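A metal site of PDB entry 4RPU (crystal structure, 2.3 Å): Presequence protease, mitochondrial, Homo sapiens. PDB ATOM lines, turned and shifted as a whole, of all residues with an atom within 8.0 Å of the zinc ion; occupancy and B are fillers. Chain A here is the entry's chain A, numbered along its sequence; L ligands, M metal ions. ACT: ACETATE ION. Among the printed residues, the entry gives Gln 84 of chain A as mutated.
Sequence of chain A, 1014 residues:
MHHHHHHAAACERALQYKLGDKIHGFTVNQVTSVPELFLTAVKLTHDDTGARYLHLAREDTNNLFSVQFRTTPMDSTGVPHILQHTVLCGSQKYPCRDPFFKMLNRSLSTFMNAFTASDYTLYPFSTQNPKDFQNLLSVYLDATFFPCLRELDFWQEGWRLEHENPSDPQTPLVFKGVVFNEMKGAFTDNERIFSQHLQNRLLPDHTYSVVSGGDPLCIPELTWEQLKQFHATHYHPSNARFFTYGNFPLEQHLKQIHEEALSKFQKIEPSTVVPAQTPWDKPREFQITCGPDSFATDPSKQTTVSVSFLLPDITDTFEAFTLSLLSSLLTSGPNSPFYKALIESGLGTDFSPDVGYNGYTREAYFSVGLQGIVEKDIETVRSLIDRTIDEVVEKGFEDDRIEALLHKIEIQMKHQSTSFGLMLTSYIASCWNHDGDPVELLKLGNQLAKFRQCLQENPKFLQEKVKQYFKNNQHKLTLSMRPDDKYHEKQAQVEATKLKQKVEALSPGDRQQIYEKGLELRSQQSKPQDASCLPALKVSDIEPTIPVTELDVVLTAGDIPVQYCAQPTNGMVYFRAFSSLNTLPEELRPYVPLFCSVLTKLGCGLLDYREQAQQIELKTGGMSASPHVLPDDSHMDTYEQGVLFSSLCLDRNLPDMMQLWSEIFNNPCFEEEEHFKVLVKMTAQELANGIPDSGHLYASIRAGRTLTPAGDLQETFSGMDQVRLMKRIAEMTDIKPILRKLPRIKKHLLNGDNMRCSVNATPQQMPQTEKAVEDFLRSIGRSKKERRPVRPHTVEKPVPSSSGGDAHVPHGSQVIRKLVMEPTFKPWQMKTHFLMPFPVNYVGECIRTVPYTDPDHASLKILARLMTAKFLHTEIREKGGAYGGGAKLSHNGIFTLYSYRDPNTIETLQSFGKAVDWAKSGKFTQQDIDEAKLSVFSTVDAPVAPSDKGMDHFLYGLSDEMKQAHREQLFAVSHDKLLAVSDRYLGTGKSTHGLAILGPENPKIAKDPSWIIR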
ATOM      1  N   HIS A  81      31.209   4.948  -5.447  1.00  0.00           N
ATOM      2  CA  HIS A  81      31.079   6.188  -6.190  1.00  0.00           C
ATOM      3  C   HIS A  81      30.785   7.355  -5.265  1.00  0.00           C
ATOM      4  O   HIS A  81      31.366   8.434  -5.374  1.00  0.00           O
ATOM      5  CB  HIS A  81      29.989   6.028  -7.241  1.00  0.00           C
ATOM      6  CG  HIS A  81      29.814   7.222  -8.127  1.00  0.00           C
ATOM      7  ND1 HIS A  81      28.669   7.455  -8.856  1.00  0.00           N
ATOM      8  CD2 HIS A  81      30.650   8.260  -8.399  1.00  0.00           C
ATOM      9  CE1 HIS A  81      28.797   8.588  -9.527  1.00  0.00           C
ATOM     10  NE2 HIS A  81      29.988   9.098  -9.263  1.00  0.00           N
ATOM     11  N   ILE A  82      29.848   7.147  -4.351  1.00  0.00           N
ATOM     12  CA  ILE A  82      29.504   8.180  -3.392  1.00  0.00           C
ATOM     13  C   ILE A  82      30.653   8.444  -2.407  1.00  0.00           C
ATOM     14  O   ILE A  82      30.907   9.591  -2.055  1.00  0.00           O
ATOM     15  CB  ILE A  82      28.204   7.798  -2.661  1.00  0.00           C
ATOM     16  CG1 ILE A  82      27.060   7.838  -3.669  1.00  0.00           C
ATOM     17  CG2 ILE A  82      27.934   8.729  -1.475  1.00  0.00           C
ATOM     18  CD1 ILE A  82      25.754   7.398  -3.133  1.00  0.00           C
ATOM     19  N   GLN A  84      33.822   8.188  -3.114  1.00  0.00           N
ATOM     20  CA  GLN A  84      34.760   8.946  -3.927  1.00  0.00           C
ATOM     21  C   GLN A  84      34.426  10.443  -3.938  1.00  0.00           C
ATOM     22  O   GLN A  84      35.324  11.277  -3.813  1.00  0.00           O
ATOM     23  CB  GLN A  84      34.792   8.387  -5.353  1.00  0.00           C
ATOM     24  CG  GLN A  84      35.655   9.196  -6.294  1.00  0.00           C
ATOM     25  CD  GLN A  84      34.947   9.545  -7.585  1.00  0.00           C
ATOM     26  OE1 GLN A  84      34.590   8.672  -8.364  1.00  0.00           O
ATOM     27  NE2 GLN A  84      34.734  10.824  -7.813  1.00  0.00           N
ATOM     28  N   HIS A  85      33.143  10.775  -4.052  1.00  0.00           N
ATOM     29  CA  HIS A  85      32.711  12.177  -3.955  1.00  0.00           C
ATOM     30  C   HIS A  85      32.949  12.749  -2.578  1.00  0.00           C
ATOM     31  O   HIS A  85      33.363  13.899  -2.443  1.00  0.00           O
ATOM     32  CB  HIS A  85      31.215  12.322  -4.294  1.00  0.00           C
ATOM     33  CG  HIS A  85      30.929  12.364  -5.760  1.00  0.00           C
ATOM     34  ND1 HIS A  85      30.361  13.453  -6.377  1.00  0.00           N
ATOM     35  CD2 HIS A  85      31.158  11.457  -6.738  1.00  0.00           C
ATOM     36  CE1 HIS A  85      30.230  13.209  -7.658  1.00  0.00           C
ATOM     37  NE2 HIS A  85      30.715  12.005  -7.915  1.00  0.00           N
ATOM     38  N   ASN A 113      40.865  15.357 -10.995  1.00  0.00           N
ATOM     39  CA  ASN A 113      39.593  14.653 -10.891  1.00  0.00           C
ATOM     40  C   ASN A 113      39.761  13.238 -10.330  1.00  0.00           C
ATOM     41  O   ASN A 113      40.854  12.775 -10.049  1.00  0.00           O
ATOM     42  CB  ASN A 113      38.995  14.407 -12.280  1.00  0.00           C
ATOM     43  CG  ASN A 113      37.467  14.570 -12.311  1.00  0.00           C
ATOM     44  OD1 ASN A 113      36.771  14.303 -11.332  1.00  0.00           O
ATOM     45  ND2 ASN A 113      36.943  15.028 -13.432  1.00  0.00           N
ATOM     46  N   ALA A 114      38.636  12.573 -10.147  1.00  0.00           N
ATOM     47  CA  ALA A 114      38.585  11.217  -9.656  1.00  0.00           C
ATOM     48  C   ALA A 114      37.485  10.470 -10.360  1.00  0.00           C
ATOM     49  O   ALA A 114      36.556  11.087 -10.883  1.00  0.00           O
ATOM     50  CB  ALA A 114      38.305  11.329  -8.176  1.00  0.00           C
ATOM     51  N   PHE A 115      37.596   9.154 -10.407  1.00  0.00           N
ATOM     52  CA  PHE A 115      36.515   8.362 -10.943  1.00  0.00           C
ATOM     53  C   PHE A 115      36.503   6.940 -10.414  1.00  0.00           C
ATOM     54  O   PHE A 115      37.508   6.421  -9.919  1.00  0.00           O
ATOM     55  CB  PHE A 115      36.565   8.356 -12.479  1.00  0.00           C
ATOM     56  CG  PHE A 115      37.861   7.866 -13.038  1.00  0.00           C
ATOM     57  CD1 PHE A 115      38.105   6.513 -13.186  1.00  0.00           C
ATOM     58  CD2 PHE A 115      38.833   8.771 -13.444  1.00  0.00           C
ATOM     59  CE1 PHE A 115      39.296   6.071 -13.716  1.00  0.00           C
ATOM     60  CE2 PHE A 115      40.020   8.341 -13.968  1.00  0.00           C
ATOM     61  CZ  PHE A 115      40.264   6.988 -14.117  1.00  0.00           C
ATOM     62  N   THR A 116      35.342   6.312 -10.569  1.00  0.00           N
ATOM     63  CA  THR A 116      35.048   5.002 -10.023  1.00  0.00           C
ATOM     64  C   THR A 116      34.720   4.046 -11.143  1.00  0.00           C
ATOM     65  O   THR A 116      33.705   4.209 -11.824  1.00  0.00           O
ATOM     66  CB  THR A 116      33.872   5.074  -9.029  1.00  0.00           C
ATOM     67  OG1 THR A 116      34.212   5.945  -7.944  1.00  0.00           O
ATOM     68  CG2 THR A 116      33.539   3.699  -8.469  1.00  0.00           C
ATOM     69  N   GLU A 157      26.298  14.942  -1.454  1.00  0.00           N
ATOM     70  CA  GLU A 157      26.893  14.275  -2.611  1.00  0.00           C
ATOM     71  C   GLU A 157      26.152  13.010  -2.995  1.00  0.00           C
ATOM     72  O   GLU A 157      26.114  12.647  -4.166  1.00  0.00           O
ATOM     73  CB  GLU A 157      28.353  13.938  -2.344  1.00  0.00           C
ATOM     74  CG  GLU A 157      29.272  15.131  -2.213  1.00  0.00           C
ATOM     75  CD  GLU A 157      29.215  16.037  -3.422  1.00  0.00           C
ATOM     76  OE1 GLU A 157      29.630  15.619  -4.522  1.00  0.00           O
ATOM     77  OE2 GLU A 157      28.725  17.181  -3.274  1.00  0.00           O
ATOM     78  N   VAL A 178      23.746  14.774  -5.403  1.00  0.00           N
ATOM     79  CA  VAL A 178      24.501  14.952  -6.631  1.00  0.00           C
ATOM     80  C   VAL A 178      24.633  13.636  -7.421  1.00  0.00           C
ATOM     81  O   VAL A 178      24.238  13.565  -8.582  1.00  0.00           O
ATOM     82  CB  VAL A 178      25.927  15.521  -6.363  1.00  0.00           C
ATOM     83  CG1 VAL A 178      26.726  15.574  -7.660  1.00  0.00           C
ATOM     84  CG2 VAL A 178      25.854  16.876  -5.703  1.00  0.00           C
ATOM     85  N   VAL A 179      25.158  12.600  -6.786  1.00  0.00           N
ATOM     86  CA  VAL A 179      25.352  11.320  -7.469  1.00  0.00           C
ATOM     87  C   VAL A 179      24.013  10.715  -7.879  1.00  0.00           C
ATOM     88  O   VAL A 179      23.901  10.053  -8.894  1.00  0.00           O
ATOM     89  CB  VAL A 179      26.127  10.321  -6.596  1.00  0.00           C
ATOM     90  CG1 VAL A 179      26.057   8.929  -7.208  1.00  0.00           C
ATOM     91  CG2 VAL A 179      27.585  10.778  -6.415  1.00  0.00           C
ATOM     92  N   PHE A 180      23.008  10.959  -7.048  1.00  0.00           N
ATOM     93  CA  PHE A 180      21.639  10.540  -7.342  1.00  0.00           C
ATOM     94  C   PHE A 180      21.228  11.007  -8.733  1.00  0.00           C
ATOM     95  O   PHE A 180      20.742  10.240  -9.550  1.00  0.00           O
ATOM     96  CB  PHE A 180      20.696  11.087  -6.255  1.00  0.00           C
ATOM     97  CG  PHE A 180      19.286  10.585  -6.339  1.00  0.00           C
ATOM     98  CD1 PHE A 180      18.991   9.279  -6.028  1.00  0.00           C
ATOM     99  CD2 PHE A 180      18.258  11.440  -6.690  1.00  0.00           C
ATOM    100  CE1 PHE A 180      17.686   8.807  -6.101  1.00  0.00           C
ATOM    101  CE2 PHE A 180      16.949  10.990  -6.761  1.00  0.00           C
ATOM    102  CZ  PHE A 180      16.668   9.670  -6.464  1.00  0.00           C
ATOM    103  N   GLU A 182      23.406  12.324 -10.966  1.00  0.00           N
ATOM    104  CA  GLU A 182      24.476  11.946 -11.870  1.00  0.00           C
ATOM    105  C   GLU A 182      24.166  10.600 -12.520  1.00  0.00           C
ATOM    106  O   GLU A 182      24.295  10.453 -13.729  1.00  0.00           O
ATOM    107  CB  GLU A 182      25.812  11.879 -11.116  1.00  0.00           C
ATOM    108  CG  GLU A 182      26.950  11.322 -11.949  1.00  0.00           C
ATOM    109  CD  GLU A 182      28.292  11.298 -11.229  1.00  0.00           C
ATOM    110  OE1 GLU A 182      28.411  11.872 -10.132  1.00  0.00           O
ATOM    111  OE2 GLU A 182      29.232  10.668 -11.757  1.00  0.00           O
ATOM    112  N   MET A 183      23.698   9.651 -11.727  1.00  0.00           N
ATOM    113  CA  MET A 183      23.429   8.318 -12.235  1.00  0.00           C
ATOM    114  C   MET A 183      22.103   8.248 -13.017  1.00  0.00           C
ATOM    115  O   MET A 183      21.995   7.478 -13.975  1.00  0.00           O
ATOM    116  CB  MET A 183      23.445   7.297 -11.092  1.00  0.00           C
ATOM    117  CG  MET A 183      24.792   7.173 -10.414  1.00  0.00           C
ATOM    118  SD  MET A 183      26.169   7.086 -11.599  1.00  0.00           S
ATOM    119  CE  MET A 183      25.785   5.568 -12.464  1.00  0.00           C
ATOM    120  N   GLY A 213      28.391   2.288  -9.915  1.00  0.00           N
ATOM    121  CA  GLY A 213      28.167   3.721  -9.884  1.00  0.00           C
ATOM    122  C   GLY A 213      26.959   4.100  -9.039  1.00  0.00           C
ATOM    123  O   GLY A 213      26.844   5.222  -8.567  1.00  0.00           O
ATOM    124  N   ARG A 877      24.452  22.791  -8.466  1.00  0.00           N
ATOM    125  CA  ARG A 877      24.896  21.442  -8.173  1.00  0.00           C
ATOM    126  C   ARG A 877      24.752  21.126  -6.690  1.00  0.00           C
ATOM    127  O   ARG A 877      24.130  20.133  -6.317  1.00  0.00           O
ATOM    128  CB  ARG A 877      26.356  21.243  -8.613  1.00  0.00           C
ATOM    129  CG  ARG A 877      27.010  20.062  -7.960  1.00  0.00           C
ATOM    130  CD  ARG A 877      28.144  19.466  -8.782  1.00  0.00           C
ATOM    131  NE  ARG A 877      28.925  18.564  -7.939  1.00  0.00           N
ATOM    132  CZ  ARG A 877      29.687  17.575  -8.374  1.00  0.00           C
ATOM    133  NH1 ARG A 877      29.816  17.324  -9.667  1.00  0.00           N
ATOM    134  NH2 ARG A 877      30.337  16.838  -7.491  1.00  0.00           N
ATOM    135  N   TYR A 883      24.324  17.603 -11.668  1.00  0.00           N
ATOM    136  CA  TYR A 883      25.673  17.097 -11.806  1.00  0.00           C
ATOM    137  C   TYR A 883      26.642  18.223 -12.134  1.00  0.00           C
ATOM    138  O   TYR A 883      27.797  18.199 -11.727  1.00  0.00           O
ATOM    139  CB  TYR A 883      25.725  15.987 -12.858  1.00  0.00           C
ATOM    140  CG  TYR A 883      27.086  15.346 -12.961  1.00  0.00           C
ATOM    141  CD1 TYR A 883      27.782  14.950 -11.827  1.00  0.00           C
ATOM    142  CD2 TYR A 883      27.659  15.098 -14.193  1.00  0.00           C
ATOM    143  CE1 TYR A 883      29.027  14.370 -11.918  1.00  0.00           C
ATOM    144  CE2 TYR A 883      28.906  14.515 -14.293  1.00  0.00           C
ATOM    145  CZ  TYR A 883      29.584  14.151 -13.152  1.00  0.00           C
ATOM    146  OH  TYR A 883      30.820  13.560 -13.240  1.00  0.00           O
ATOM    147  N   ARG A 901      22.573  17.356 -16.316  1.00  0.00           N
ATOM    148  CA  ARG A 901      21.871  16.374 -15.482  1.00  0.00           C
ATOM    149  C   ARG A 901      21.204  17.067 -14.283  1.00  0.00           C
ATOM    150  O   ARG A 901      21.469  16.761 -13.131  1.00  0.00           O
ATOM    151  CB  ARG A 901      22.818  15.274 -15.002  1.00  0.00           C
ATOM    152  CG  ARG A 901      23.499  14.526 -16.149  1.00  0.00           C
ATOM    153  CD  ARG A 901      24.356  13.366 -15.678  1.00  0.00           C
ATOM    154  NE  ARG A 901      25.198  12.918 -16.774  1.00  0.00           N
ATOM    155  CZ  ARG A 901      26.126  11.969 -16.710  1.00  0.00           C
ATOM    156  NH1 ARG A 901      26.359  11.319 -15.582  1.00  0.00           N
ATOM    157  NH2 ARG A 901      26.814  11.672 -17.797  1.00  0.00           N
HETATM  158  C   ACT L   1      32.643  11.639 -10.838  1.00  0.00           C
HETATM  159  O   ACT L   1      31.677  12.427 -10.676  1.00  0.00           O
HETATM  160  OXT ACT L   1      32.593  10.556 -10.212  1.00  0.00           O
HETATM  161  CH3 ACT L   1      33.791  11.960 -11.739  1.00  0.00           C
HETATM  162 ZN    ZN M   1      30.410  11.017  -9.747  1.00  0.00          ZN
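The backbone carbonyl oxygen of Glu 182 is in hydrogen-bond range of the guanidinium group of Arg 901 (2.9 Å). A ring nitrogen (ND1) of His 85 lies within hydrogen-bond range of the side-chain carboxylate (OE1) of Glu 157 (2.9 Å). ND1 of His 81 sits close to SD of Met 183 (3.7 Å). ND1 of His 81 is in hydrogen-bond range of O of Gly 213 (2.9 Å).
Within 4 Å of the zinc ion: His 81, His 85 and Glu 182. Along chain A the residues within 4 Å of the zinc ion span positions 81 to 182.
The zinc ion is bound by a ring nitrogen (NE2) of His 81 (2.0 Å), a ring nitrogen (NE2) of His 85 (2.1 Å), an oxygen (O) of the ligand (2.1 Å), the side-chain carboxylate (OE1) of Glu 182 (2.2 Å), an oxygen (OXT) of the ligand (2.3 Å) and the side-chain carboxylate (OE2) of Glu 182 (2.4 Å). The zinc ion has six donor atoms within binding distance.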
